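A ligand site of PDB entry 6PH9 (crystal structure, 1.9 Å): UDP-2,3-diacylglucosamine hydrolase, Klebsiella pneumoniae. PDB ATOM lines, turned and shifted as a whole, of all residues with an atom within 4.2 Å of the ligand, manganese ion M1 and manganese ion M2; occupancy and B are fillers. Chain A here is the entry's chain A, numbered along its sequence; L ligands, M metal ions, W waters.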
ATOM      1  N   ASP A   9      -4.789   0.921  19.532  1.00  0.00           N
ATOM      2  CA  ASP A   9      -5.919   1.707  19.043  1.00  0.00           C
ATOM      3  C   ASP A   9      -5.908   1.857  17.528  1.00  0.00           C
ATOM      4  O   ASP A   9      -6.142   2.946  16.984  1.00  0.00           O
ATOM      5  CB  ASP A   9      -5.965   3.074  19.735  1.00  0.00           C
ATOM      6  CG  ASP A   9      -6.140   2.948  21.238  1.00  0.00           C
ATOM      7  OD1 ASP A   9      -7.212   2.499  21.674  1.00  0.00           O
ATOM      8  OD2 ASP A   9      -5.179   3.274  21.979  1.00  0.00           O
ATOM      9  N   HIS A  11      -8.065   0.057  15.729  1.00  0.00           N
ATOM     10  CA  HIS A  11      -9.499  -0.040  15.459  1.00  0.00           C
ATOM     11  C   HIS A  11      -9.763  -0.508  14.035  1.00  0.00           C
ATOM     12  O   HIS A  11     -10.569   0.060  13.292  1.00  0.00           O
ATOM     13  CB  HIS A  11     -10.183   1.300  15.737  1.00  0.00           C
ATOM     14  CG  HIS A  11     -10.258   1.665  17.193  1.00  0.00           C
ATOM     15  ND1 HIS A  11     -11.355   1.363  17.974  1.00  0.00           N
ATOM     16  CD2 HIS A  11      -9.377   2.303  17.997  1.00  0.00           C
ATOM     17  CE1 HIS A  11     -11.143   1.802  19.203  1.00  0.00           C
ATOM     18  NE2 HIS A  11      -9.952   2.370  19.247  1.00  0.00           N
ATOM     19  N   ASP A  42      -7.253  -2.712  21.511  1.00  0.00           N
ATOM     20  CA  ASP A  42      -8.010  -2.060  20.446  1.00  0.00           C
ATOM     21  C   ASP A  42      -7.311  -2.201  19.105  1.00  0.00           C
ATOM     22  O   ASP A  42      -7.222  -1.257  18.314  1.00  0.00           O
ATOM     23  CB  ASP A  42      -8.281  -0.588  20.772  1.00  0.00           C
ATOM     24  CG  ASP A  42      -9.276  -0.425  21.908  1.00  0.00           C
ATOM     25  OD1 ASP A  42      -9.817  -1.440  22.376  1.00  0.00           O
ATOM     26  OD2 ASP A  42      -9.519   0.727  22.312  1.00  0.00           O
ATOM     27  N   TRP A  47     -14.654  -7.031  18.579  1.00  0.00           N
ATOM     28  CA  TRP A  47     -14.404  -8.459  18.524  1.00  0.00           C
ATOM     29  C   TRP A  47     -15.567  -9.185  19.191  1.00  0.00           C
ATOM     30  O   TRP A  47     -15.873  -8.915  20.355  1.00  0.00           O
ATOM     31  CB  TRP A  47     -13.093  -8.833  19.219  1.00  0.00           C
ATOM     32  CG  TRP A  47     -12.549 -10.178  18.820  1.00  0.00           C
ATOM     33  CD1 TRP A  47     -12.734 -11.364  19.482  1.00  0.00           C
ATOM     34  CD2 TRP A  47     -11.711 -10.476  17.695  1.00  0.00           C
ATOM     35  NE1 TRP A  47     -12.082 -12.376  18.822  1.00  0.00           N
ATOM     36  CE2 TRP A  47     -11.437 -11.863  17.729  1.00  0.00           C
ATOM     37  CE3 TRP A  47     -11.173  -9.712  16.661  1.00  0.00           C
ATOM     38  CZ2 TRP A  47     -10.650 -12.499  16.764  1.00  0.00           C
ATOM     39  CZ3 TRP A  47     -10.390 -10.341  15.702  1.00  0.00           C
ATOM     40  CH2 TRP A  47     -10.133 -11.715  15.760  1.00  0.00           C
ATOM     41  N   ASN A  80     -10.704  -2.388  25.321  1.00  0.00           N
ATOM     42  CA  ASN A  80     -12.144  -2.381  25.579  1.00  0.00           C
ATOM     43  C   ASN A  80     -12.937  -2.804  24.352  1.00  0.00           C
ATOM     44  O   ASN A  80     -14.119  -3.158  24.493  1.00  0.00           O
ATOM     45  CB  ASN A  80     -12.589  -1.010  26.061  1.00  0.00           C
ATOM     46  CG  ASN A  80     -12.347   0.080  25.039  1.00  0.00           C
ATOM     47  OD1 ASN A  80     -11.201   0.487  24.821  1.00  0.00           O
ATOM     48  ND2 ASN A  80     -13.411   0.561  24.412  1.00  0.00           N
ATOM     49  N   ARG A  81     -12.329  -2.776  23.174  1.00  0.00           N
ATOM     50  CA  ARG A  81     -13.011  -3.202  21.950  1.00  0.00           C
ATOM     51  C   ARG A  81     -12.826  -4.677  21.645  1.00  0.00           C
ATOM     52  O   ARG A  81     -13.709  -5.287  21.037  1.00  0.00           O
ATOM     53  CB  ARG A  81     -12.519  -2.385  20.757  1.00  0.00           C
ATOM     54  CG  ARG A  81     -12.779  -0.889  20.856  1.00  0.00           C
ATOM     55  CD  ARG A  81     -14.270  -0.583  20.887  1.00  0.00           C
ATOM     56  NE  ARG A  81     -14.505   0.862  20.818  1.00  0.00           N
ATOM     57  CZ  ARG A  81     -14.509   1.557  19.689  1.00  0.00           C
ATOM     58  NH1 ARG A  81     -14.297   0.944  18.538  1.00  0.00           N
ATOM     59  NH2 ARG A  81     -14.725   2.866  19.712  1.00  0.00           N
ATOM     60  N   PHE A  83     -11.661  -7.360  23.939  1.00  0.00           N
ATOM     61  CA  PHE A  83     -11.343  -8.185  25.106  1.00  0.00           C
ATOM     62  C   PHE A  83     -11.693  -9.651  24.896  1.00  0.00           C
ATOM     63  O   PHE A  83     -11.263 -10.501  25.694  1.00  0.00           O
ATOM     64  CB  PHE A  83     -12.050  -7.647  26.349  1.00  0.00           C
ATOM     65  CG  PHE A  83     -13.546  -7.471  26.174  1.00  0.00           C
ATOM     66  CD1 PHE A  83     -14.414  -8.519  26.437  1.00  0.00           C
ATOM     67  CD2 PHE A  83     -14.058  -6.260  25.755  1.00  0.00           C
ATOM     68  CE1 PHE A  83     -15.781  -8.359  26.276  1.00  0.00           C
ATOM     69  CE2 PHE A  83     -15.428  -6.093  25.599  1.00  0.00           C
ATOM     70  CZ  PHE A  83     -16.293  -7.148  25.857  1.00  0.00           C
ATOM     71  N   LEU A  84     -12.465  -9.979  23.862  1.00  0.00           N
ATOM     72  CA  LEU A  84     -12.829 -11.369  23.593  1.00  0.00           C
ATOM     73  C   LEU A  84     -11.823 -12.097  22.715  1.00  0.00           C
ATOM     74  O   LEU A  84     -12.028 -13.284  22.415  1.00  0.00           O
ATOM     75  CB  LEU A  84     -14.220 -11.437  22.945  1.00  0.00           C
ATOM     76  CG  LEU A  84     -15.413 -11.065  23.829  1.00  0.00           C
ATOM     77  CD1 LEU A  84     -16.714 -11.137  23.046  1.00  0.00           C
ATOM     78  CD2 LEU A  84     -15.468 -11.965  25.055  1.00  0.00           C
ATOM     79  N   HIS A 115      -3.637  -1.313  28.524  1.00  0.00           N
ATOM     80  CA  HIS A 115      -4.430  -0.607  27.524  1.00  0.00           C
ATOM     81  C   HIS A 115      -4.714   0.820  27.959  1.00  0.00           C
ATOM     82  O   HIS A 115      -4.633   1.757  27.154  1.00  0.00           O
ATOM     83  CB  HIS A 115      -5.733  -1.337  27.248  1.00  0.00           C
ATOM     84  CG  HIS A 115      -6.587  -0.642  26.223  1.00  0.00           C
ATOM     85  ND1 HIS A 115      -6.153  -0.408  24.940  1.00  0.00           N
ATOM     86  CD2 HIS A 115      -7.825  -0.100  26.313  1.00  0.00           C
ATOM     87  CE1 HIS A 115      -7.097   0.240  24.270  1.00  0.00           C
ATOM     88  NE2 HIS A 115      -8.118   0.437  25.087  1.00  0.00           N
ATOM     89  N   ASP A 123     -14.827   7.183  35.995  1.00  0.00           N
ATOM     90  CA  ASP A 123     -15.946   6.770  35.163  1.00  0.00           C
ATOM     91  C   ASP A 123     -16.531   5.493  35.762  1.00  0.00           C
ATOM     92  O   ASP A 123     -16.295   4.380  35.300  1.00  0.00           O
ATOM     93  CB  ASP A 123     -15.492   6.561  33.719  1.00  0.00           C
ATOM     94  CG  ASP A 123     -16.655   6.524  32.740  1.00  0.00           C
ATOM     95  OD1 ASP A 123     -17.799   6.277  33.160  1.00  0.00           O
ATOM     96  OD2 ASP A 123     -16.409   6.760  31.533  1.00  0.00           O
ATOM     97  N   GLY A 125     -19.513   4.410  35.704  1.00  0.00           N
ATOM     98  CA  GLY A 125     -20.359   3.698  34.751  1.00  0.00           C
ATOM     99  C   GLY A 125     -19.558   2.748  33.883  1.00  0.00           C
ATOM    100  O   GLY A 125     -19.929   1.586  33.714  1.00  0.00           O
ATOM    101  N   TYR A 126     -18.445   3.227  33.322  1.00  0.00           N
ATOM    102  CA  TYR A 126     -17.631   2.366  32.467  1.00  0.00           C
ATOM    103  C   TYR A 126     -17.087   1.180  33.238  1.00  0.00           C
ATOM    104  O   TYR A 126     -17.148   0.041  32.747  1.00  0.00           O
ATOM    105  CB  TYR A 126     -16.472   3.149  31.846  1.00  0.00           C
ATOM    106  CG  TYR A 126     -15.489   2.185  31.207  1.00  0.00           C
ATOM    107  CD1 TYR A 126     -15.863   1.457  30.089  1.00  0.00           C
ATOM    108  CD2 TYR A 126     -14.236   1.960  31.767  1.00  0.00           C
ATOM    109  CE1 TYR A 126     -14.995   0.551  29.515  1.00  0.00           C
ATOM    110  CE2 TYR A 126     -13.365   1.046  31.187  1.00  0.00           C
ATOM    111  CZ  TYR A 126     -13.750   0.343  30.064  1.00  0.00           C
ATOM    112  OH  TYR A 126     -12.885  -0.558  29.482  1.00  0.00           O
ATOM    113  N   PHE A 129     -19.616  -1.485  33.635  1.00  0.00           N
ATOM    114  CA  PHE A 129     -19.722  -2.218  32.369  1.00  0.00           C
ATOM    115  C   PHE A 129     -18.544  -3.153  32.182  1.00  0.00           C
ATOM    116  O   PHE A 129     -18.704  -4.316  31.788  1.00  0.00           O
ATOM    117  CB  PHE A 129     -19.816  -1.213  31.211  1.00  0.00           C
ATOM    118  CG  PHE A 129     -19.864  -1.858  29.861  1.00  0.00           C
ATOM    119  CD1 PHE A 129     -21.050  -2.342  29.340  1.00  0.00           C
ATOM    120  CD2 PHE A 129     -18.707  -1.966  29.083  1.00  0.00           C
ATOM    121  CE1 PHE A 129     -21.104  -2.928  28.087  1.00  0.00           C
ATOM    122  CE2 PHE A 129     -18.752  -2.548  27.831  1.00  0.00           C
ATOM    123  CZ  PHE A 129     -19.952  -3.026  27.329  1.00  0.00           C
ATOM    124  N   VAL A 133     -18.632  -7.389  31.391  1.00  0.00           N
ATOM    125  CA  VAL A 133     -18.191  -8.018  30.155  1.00  0.00           C
ATOM    126  C   VAL A 133     -16.905  -8.805  30.326  1.00  0.00           C
ATOM    127  O   VAL A 133     -16.485  -9.508  29.398  1.00  0.00           O
ATOM    128  CB  VAL A 133     -18.036  -6.976  29.034  1.00  0.00           C
ATOM    129  CG1 VAL A 133     -19.377  -6.284  28.775  1.00  0.00           C
ATOM    130  CG2 VAL A 133     -16.966  -5.963  29.387  1.00  0.00           C
ATOM    131  N   ILE A 138     -20.475 -14.788  31.766  1.00  0.00           N
ATOM    132  CA  ILE A 138     -21.175 -13.881  30.860  1.00  0.00           C
ATOM    133  C   ILE A 138     -20.511 -13.901  29.494  1.00  0.00           C
ATOM    134  O   ILE A 138     -21.194 -13.854  28.455  1.00  0.00           O
ATOM    135  CB  ILE A 138     -21.210 -12.467  31.458  1.00  0.00           C
ATOM    136  CG1 ILE A 138     -22.023 -12.458  32.762  1.00  0.00           C
ATOM    137  CG2 ILE A 138     -21.814 -11.479  30.466  1.00  0.00           C
ATOM    138  CD1 ILE A 138     -22.084 -11.105  33.426  1.00  0.00           C
ATOM    139  N   GLN A 139     -19.178 -13.965  29.446  1.00  0.00           N
ATOM    140  CA  GLN A 139     -18.482 -14.102  28.169  1.00  0.00           C
ATOM    141  C   GLN A 139     -18.839 -15.409  27.481  1.00  0.00           C
ATOM    142  O   GLN A 139     -19.091 -15.432  26.270  1.00  0.00           O
ATOM    143  CB  GLN A 139     -16.972 -14.001  28.374  1.00  0.00           C
ATOM    144  CG  GLN A 139     -16.484 -12.665  28.888  1.00  0.00           C
ATOM    145  CD  GLN A 139     -14.967 -12.602  28.948  1.00  0.00           C
ATOM    146  OE1 GLN A 139     -14.296 -13.632  29.001  1.00  0.00           O
ATOM    147  NE2 GLN A 139     -14.430 -11.392  28.957  1.00  0.00           N
ATOM    148  N   PHE A 142     -22.300 -15.111  25.912  1.00  0.00           N
ATOM    149  CA  PHE A 142     -22.273 -14.339  24.678  1.00  0.00           C
ATOM    150  C   PHE A 142     -21.696 -15.163  23.528  1.00  0.00           C
ATOM    151  O   PHE A 142     -22.251 -15.177  22.418  1.00  0.00           O
ATOM    152  CB  PHE A 142     -21.447 -13.064  24.895  1.00  0.00           C
ATOM    153  CG  PHE A 142     -21.294 -12.207  23.664  1.00  0.00           C
ATOM    154  CD1 PHE A 142     -22.230 -11.222  23.372  1.00  0.00           C
ATOM    155  CD2 PHE A 142     -20.195 -12.356  22.831  1.00  0.00           C
ATOM    156  CE1 PHE A 142     -22.084 -10.422  22.252  1.00  0.00           C
ATOM    157  CE2 PHE A 142     -20.043 -11.544  21.716  1.00  0.00           C
ATOM    158  CZ  PHE A 142     -20.989 -10.587  21.422  1.00  0.00           C
ATOM    159  N   ILE A 153     -25.928  -7.371  19.220  1.00  0.00           N
ATOM    160  CA  ILE A 153     -25.578  -6.921  20.561  1.00  0.00           C
ATOM    161  C   ILE A 153     -24.399  -5.949  20.514  1.00  0.00           C
ATOM    162  O   ILE A 153     -24.396  -4.921  21.194  1.00  0.00           O
ATOM    163  CB  ILE A 153     -25.276  -8.134  21.467  1.00  0.00           C
ATOM    164  CG1 ILE A 153     -26.539  -8.951  21.702  1.00  0.00           C
ATOM    165  CG2 ILE A 153     -24.686  -7.679  22.793  1.00  0.00           C
ATOM    166  CD1 ILE A 153     -26.283 -10.323  22.287  1.00  0.00           C
ATOM    167  N   ALA A 154     -23.386  -6.269  19.697  1.00  0.00           N
ATOM    168  CA  ALA A 154     -22.246  -5.378  19.553  1.00  0.00           C
ATOM    169  C   ALA A 154     -22.678  -4.030  18.978  1.00  0.00           C
ATOM    170  O   ALA A 154     -22.168  -2.977  19.389  1.00  0.00           O
ATOM    171  CB  ALA A 154     -21.180  -6.023  18.673  1.00  0.00           C
ATOM    172  N   MET A 157     -24.277  -2.023  21.793  1.00  0.00           N
ATOM    173  CA  MET A 157     -23.261  -1.531  22.724  1.00  0.00           C
ATOM    174  C   MET A 157     -22.500  -0.350  22.151  1.00  0.00           C
ATOM    175  O   MET A 157     -22.217   0.623  22.853  1.00  0.00           O
ATOM    176  CB  MET A 157     -22.300  -2.664  23.089  1.00  0.00           C
ATOM    177  CG  MET A 157     -22.895  -3.731  23.995  1.00  0.00           C
ATOM    178  SD  MET A 157     -21.747  -5.096  24.255  1.00  0.00           S
ATOM    179  CE  MET A 157     -22.603  -6.033  25.525  1.00  0.00           C
ATOM    180  N   ARG A 158     -22.131  -0.425  20.869  1.00  0.00           N
ATOM    181  CA  ARG A 158     -21.441   0.698  20.221  1.00  0.00           C
ATOM    182  C   ARG A 158     -22.321   1.939  20.197  1.00  0.00           C
ATOM    183  O   ARG A 158     -21.847   3.047  20.472  1.00  0.00           O
ATOM    184  CB  ARG A 158     -21.013   0.310  18.809  1.00  0.00           C
ATOM    185  CG  ARG A 158     -19.959  -0.784  18.742  1.00  0.00           C
ATOM    186  CD  ARG A 158     -18.633  -0.316  19.323  1.00  0.00           C
ATOM    187  NE  ARG A 158     -18.162   0.919  18.706  1.00  0.00           N
ATOM    188  CZ  ARG A 158     -17.941   2.047  19.373  1.00  0.00           C
ATOM    189  NH1 ARG A 158     -18.133   2.098  20.676  1.00  0.00           N
ATOM    190  NH2 ARG A 158     -17.508   3.129  18.725  1.00  0.00           N
ATOM    191  N   ASP A 160     -24.822   2.765  22.250  1.00  0.00           N
ATOM    192  CA  ASP A 160     -24.976   3.322  23.590  1.00  0.00           C
ATOM    193  C   ASP A 160     -23.682   3.906  24.117  1.00  0.00           C
ATOM    194  O   ASP A 160     -23.711   4.883  24.884  1.00  0.00           O
ATOM    195  CB  ASP A 160     -25.495   2.236  24.535  1.00  0.00           C
ATOM    196  CG  ASP A 160     -26.893   1.779  24.184  1.00  0.00           C
ATOM    197  OD1 ASP A 160     -27.544   2.440  23.358  1.00  0.00           O
ATOM    198  OD2 ASP A 160     -27.329   0.753  24.736  1.00  0.00           O
ATOM    199  N   SER A 161     -22.531   3.336  23.736  1.00  0.00           N
ATOM    200  CA  SER A 161     -21.256   3.914  24.133  1.00  0.00           C
ATOM    201  C   SER A 161     -21.066   5.302  23.541  1.00  0.00           C
ATOM    202  O   SER A 161     -20.717   6.250  24.246  1.00  0.00           O
ATOM    203  CB  SER A 161     -20.114   2.987  23.710  1.00  0.00           C
ATOM    204  OG  SER A 161     -18.863   3.498  24.146  1.00  0.00           O
ATOM    205  N   ALA A 164     -23.356   7.632  25.460  1.00  0.00           N
ATOM    206  CA  ALA A 164     -22.853   7.944  26.797  1.00  0.00           C
ATOM    207  C   ALA A 164     -21.597   8.799  26.742  1.00  0.00           C
ATOM    208  O   ALA A 164     -21.380   9.627  27.639  1.00  0.00           O
ATOM    209  CB  ALA A 164     -22.578   6.647  27.565  1.00  0.00           C
ATOM    210  N   ASN A 165     -20.774   8.627  25.708  1.00  0.00           N
ATOM    211  CA  ASN A 165     -19.572   9.456  25.581  1.00  0.00           C
ATOM    212  C   ASN A 165     -19.926  10.895  25.241  1.00  0.00           C
ATOM    213  O   ASN A 165     -19.175  11.811  25.577  1.00  0.00           O
ATOM    214  CB  ASN A 165     -18.651   8.861  24.519  1.00  0.00           C
ATOM    215  CG  ASN A 165     -18.071   7.529  24.931  1.00  0.00           C
ATOM    216  OD1 ASN A 165     -17.948   7.239  26.124  1.00  0.00           O
ATOM    217  ND2 ASN A 165     -17.718   6.710  23.954  1.00  0.00           N
ATOM    218  N   LYS A 168     -21.350  12.408  28.671  1.00  0.00           N
ATOM    219  CA  LYS A 168     -20.404  12.436  29.776  1.00  0.00           C
ATOM    220  C   LYS A 168     -19.394  13.557  29.577  1.00  0.00           C
ATOM    221  O   LYS A 168     -19.049  13.910  28.436  1.00  0.00           O
ATOM    222  CB  LYS A 168     -19.674  11.092  29.901  1.00  0.00           C
ATOM    223  CG  LYS A 168     -20.379  10.093  30.806  1.00  0.00           C
ATOM    224  CD  LYS A 168     -19.495   8.868  31.066  1.00  0.00           C
ATOM    225  CE  LYS A 168     -19.355   8.009  29.825  1.00  0.00           C
ATOM    226  NZ  LYS A 168     -18.935   6.616  30.161  1.00  0.00           N
ATOM    227  N   MET A 173     -14.194  11.147  32.221  1.00  0.00           N
ATOM    228  CA  MET A 173     -13.788  10.028  31.385  1.00  0.00           C
ATOM    229  C   MET A 173     -12.282   9.902  31.205  1.00  0.00           C
ATOM    230  O   MET A 173     -11.805   8.814  30.846  1.00  0.00           O
ATOM    231  CB  MET A 173     -14.424  10.142  29.991  1.00  0.00           C
ATOM    232  CG  MET A 173     -15.942  10.150  29.997  1.00  0.00           C
ATOM    233  SD  MET A 173     -16.623   9.797  28.362  1.00  0.00           S
ATOM    234  CE  MET A 173     -15.990  11.184  27.421  1.00  0.00           C
ATOM    235  N   HIS A 196      -5.776   3.782  24.560  1.00  0.00           N
ATOM    236  CA  HIS A 196      -7.180   3.996  24.884  1.00  0.00           C
ATOM    237  C   HIS A 196      -7.661   5.445  24.705  1.00  0.00           C
ATOM    238  O   HIS A 196      -8.707   5.677  24.104  1.00  0.00           O
ATOM    239  CB  HIS A 196      -7.505   3.551  26.311  1.00  0.00           C
ATOM    240  CG  HIS A 196      -8.948   3.684  26.668  1.00  0.00           C
ATOM    241  ND1 HIS A 196      -9.945   2.986  26.016  1.00  0.00           N
ATOM    242  CD2 HIS A 196      -9.577   4.455  27.586  1.00  0.00           C
ATOM    243  CE1 HIS A 196     -11.115   3.312  26.521  1.00  0.00           C
ATOM    244  NE2 HIS A 196     -10.928   4.203  27.475  1.00  0.00           N
ATOM    245  N   HIS A 198      -6.396   8.032  23.045  1.00  0.00           N
ATOM    246  CA  HIS A 198      -6.193   8.617  21.711  1.00  0.00           C
ATOM    247  C   HIS A 198      -5.634  10.038  21.790  1.00  0.00           C
ATOM    248  O   HIS A 198      -5.884  10.858  20.912  1.00  0.00           O
ATOM    249  CB  HIS A 198      -7.481   8.611  20.880  1.00  0.00           C
ATOM    250  CG  HIS A 198      -8.080   7.250  20.693  1.00  0.00           C
ATOM    251  ND1 HIS A 198      -9.150   7.016  19.846  1.00  0.00           N
ATOM    252  CD2 HIS A 198      -7.770   6.047  21.244  1.00  0.00           C
ATOM    253  CE1 HIS A 198      -9.469   5.742  19.883  1.00  0.00           C
ATOM    254  NE2 HIS A 198      -8.651   5.123  20.724  1.00  0.00           N
HETATM  255  O1  LIG L   1     -14.519   4.299  22.429  1.00  0.00           O
HETATM  256  P1  LIG L   1     -15.745   3.660  23.046  1.00  0.00           P
HETATM  257  O2  LIG L   1     -16.972   4.091  22.290  1.00  0.00           O
HETATM  258  O3  LIG L   1     -15.612   2.153  22.988  1.00  0.00           O
HETATM  259  O4  LIG L   1     -15.873   4.139  24.620  1.00  0.00           O
HETATM  260  C1  LIG L   1     -15.211   3.429  25.594  1.00  0.00           C
HETATM  261  C2  LIG L   1     -16.244   2.921  26.593  1.00  0.00           C
HETATM  262  N1  LIG L   1     -17.241   2.082  25.881  1.00  0.00           N
HETATM  263  C3  LIG L   1     -16.965   0.669  25.696  1.00  0.00           C
HETATM  264  C4  LIG L   1     -17.978  -0.206  24.967  1.00  0.00           C
HETATM  265  C5  LIG L   1     -17.335  -0.747  23.704  1.00  0.00           C
HETATM  266  O5  LIG L   1     -17.135   0.291  22.782  1.00  0.00           O
HETATM  267  C6  LIG L   1     -18.258  -1.792  23.088  1.00  0.00           C
HETATM  268  C7  LIG L   1     -17.427  -2.640  22.117  1.00  0.00           C
HETATM  269  C8  LIG L   1     -18.256  -3.838  21.682  1.00  0.00           C
HETATM  270  C9  LIG L   1     -17.409  -5.103  21.846  1.00  0.00           C
HETATM  271  C10 LIG L   1     -18.059  -6.233  21.068  1.00  0.00           C
HETATM  272  C11 LIG L   1     -19.223  -6.771  21.895  1.00  0.00           C
HETATM  273  C12 LIG L   1     -18.663  -7.780  22.887  1.00  0.00           C
HETATM  274  C13 LIG L   1     -19.610  -7.909  24.075  1.00  0.00           C
HETATM  275  C14 LIG L   1     -19.253  -9.168  24.843  1.00  0.00           C
HETATM  276  C15 LIG L   1     -20.095  -9.263  26.107  1.00  0.00           C
HETATM  277  C16 LIG L   1     -19.648 -10.479  26.911  1.00  0.00           C
HETATM  278  O6  LIG L   1     -15.954   0.206  26.098  1.00  0.00           O
HETATM  279  C17 LIG L   1     -16.948   4.040  27.272  1.00  0.00           C
HETATM  280  C18 LIG L   1     -16.005   4.996  27.878  1.00  0.00           C
HETATM  281  C19 LIG L   1     -14.970   5.478  26.862  1.00  0.00           C
HETATM  282  O7  LIG L   1     -14.255   4.310  26.258  1.00  0.00           O
HETATM  283  C20 LIG L   1     -13.963   6.319  27.560  1.00  0.00           C
HETATM  284  O8  LIG L   1     -13.225   5.518  28.435  1.00  0.00           O
HETATM  285  O9  LIG L   1     -16.765   6.143  28.337  1.00  0.00           O
HETATM  286  O10 LIG L   1     -17.772   3.486  28.342  1.00  0.00           O
HETATM  287  C21 LIG L   1     -19.149   3.644  28.159  1.00  0.00           C
HETATM  288  O11 LIG L   1     -19.560   4.545  27.504  1.00  0.00           O
HETATM  289  C22 LIG L   1     -20.112   2.657  28.807  1.00  0.00           C
HETATM  290  C23 LIG L   1     -21.250   3.407  29.495  1.00  0.00           C
HETATM  291  O12 LIG L   1     -20.751   4.199  30.532  1.00  0.00           O
HETATM  292  C24 LIG L   1     -22.231   2.364  30.043  1.00  0.00           C
HETATM  293  C25 LIG L   1     -22.810   1.603  28.856  1.00  0.00           C
HETATM  294  C26 LIG L   1     -23.432   0.290  29.300  1.00  0.00           C
HETATM  295  C27 LIG L   1     -24.780   0.129  28.609  1.00  0.00           C
HETATM  296  C28 LIG L   1     -24.619  -0.751  27.373  1.00  0.00           C
HETATM  297  C29 LIG L   1     -25.220  -2.133  27.652  1.00  0.00           C
HETATM  298  C30 LIG L   1     -25.839  -2.693  26.379  1.00  0.00           C
HETATM  299  C31 LIG L   1     -26.311  -4.112  26.648  1.00  0.00           C
HETATM  300  C32 LIG L   1     -27.202  -4.609  25.512  1.00  0.00           C
HETATM  301  C33 LIG L   1     -27.462  -6.105  25.677  1.00  0.00           C
HETATM  302  C34 LIG L   1     -28.287  -6.625  24.508  1.00  0.00           C
HETATM  303 MN    MN M   1      -9.688   1.622  24.216  1.00  0.00          MN
HETATM  304 MN    MN M   2      -8.965   2.943  21.179  1.00  0.00          MN
HETATM  305  O   HOH W   1     -12.380   2.705  22.519  1.00  0.00           O
HETATM  306  O   HOH W   2     -13.661   6.532  30.878  1.00  0.00           O
HETATM  307  O   HOH W   3     -17.258   5.463  19.969  1.00  0.00           O
HETATM  308  O   HOH W   4     -15.794  -2.656  26.508  1.00  0.00           O
HETATM  309  O   HOH W   5     -12.876   5.783  23.656  1.00  0.00           O
HETATM  310  O   HOH W   6      -9.980   3.119  23.069  1.00  0.00           O
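NZ of Lys 168 sits at hydrogen-bond distance from O9 of the ligand (2.9 Å).
OD1 of Asn 165 lies within hydrogen-bond range of O9 of the ligand, at 2.7 Å.
A ring nitrogen (NE2) of His 196 sits at hydrogen-bond distance from an oxygen (O8) of the ligand (2.8 Å).
OD2 of Asp 123 sits at hydrogen-bond distance from O9 of the ligand (3.3 Å).
The side-chain sulfur (SD) of Met 173 is in hydrogen-bond range of an oxygen (O9) of the ligand, at 3.7 Å.
The side-chain amide nitrogen (ND2) of Asn 80 is in hydrogen-bond range of an oxygen (O3) of the ligand (3.1 Å).
O3 of the ligand is in salt-bridge range of NE of Arg 81, 2.8 Å away.
The side-chain hydroxyl (OG) of Ser 161 sits at hydrogen-bond distance from an oxygen (O2) of the ligand, at 2.7 Å.
An oxygen (O2) of the ligand lies within salt-bridge range of the guanidinium group (NH1) of Arg 158, at 2.8 Å.
NZ of Lys 168 lies within salt-bridge range of OD2 of Asp 123, 2.9 Å away.
The side-chain carboxylate (OD1) of Asp 42 lies within hydrogen-bond range of the backbone NH (N) of Arg 81 (3.0 Å).
The backbone NH (N) of Trp 47 is in hydrogen-bond range of the backbone carbonyl oxygen (O) of Arg 81, 3.2 Å away.
The side-chain carboxylate (OD1) of Asp 123 lies within hydrogen-bond range of the backbone NH (N) of Tyr 126, 3.1 Å away.
NE2 of His 198 sits close to O of His 196 (3.4 Å).
NH1 of Arg 81 lies within hydrogen-bond range of ND1 of His 11, 3.0 Å away.
The side-chain amide nitrogen of Asn 165 sits close to the backbone carbonyl oxygen of Ser 161, 3.0 Å away.
The side-chain carboxylate (OD2) of Asp 9 lies within hydrogen-bond range of the backbone NH (N) of His 196 (2.7 Å).
Merely in contact with the ligand: Trp 47, Phe 83, Leu 84, Gly 125, Tyr 126, Phe 129, Phe 142, Ala 154, Met 157 and Ala 164.
Of the 29 residues printed, 19 come within 4 Å of the ligand.
Within 4 Å of manganese ion M1: Asp 9, Asp 42, Asn 80, His 115 and His 196.
Along chain A the residues within 4 Å of manganese ion M1 span positions 9 to 196.
The nearest printed residue that does not touch manganese ion M1 is His 11 (5.0 Å).
Of the 29 residues printed, 4 come within 4 Å of manganese ion M2.
The nearest printed residue that does not touch manganese ion M2 is His 196 (4.01 Å).
Manganese ion M1 is bound by water W6, the side-chain amide oxygen (OD1) of Asn 80, the side-chain carboxylate (OD2) of Asp 42, a ring nitrogen (NE2) of His 115 and a ring nitrogen (ND1) of His 196.
Manganese ion M1 has five donor atoms within binding distance.
Manganese ion M2 is bound by the side-chain carboxylate (OD1) of Asp 9, water W6, a ring nitrogen (NE2) of His 11, a ring nitrogen (NE2) of His 198 and the side-chain carboxylate (OD2) of Asp 42.
Manganese ion M2 has five donor atoms within binding distance.
Water W1 lies within hydrogen-bond range of O1 of the ligand, ND2 of Asn 80 and NE of Arg 81.
Water W2 lies within hydrogen-bond range of an oxygen (O8) of the ligand (2.7 Å), the side-chain carboxylate of Asp 123 (2.8 Å) and the backbone carbonyl oxygen of Met 173 (2.9 Å).
Water W3 bridges the guanidinium group (NH2) of Arg 158 (2.7 Å) and an oxygen (O2) of the ligand (2.7 Å).
Water W4 lies within hydrogen-bond range of O of Asn 80 (2.7 Å) and O6 of the ligand (2.9 Å).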
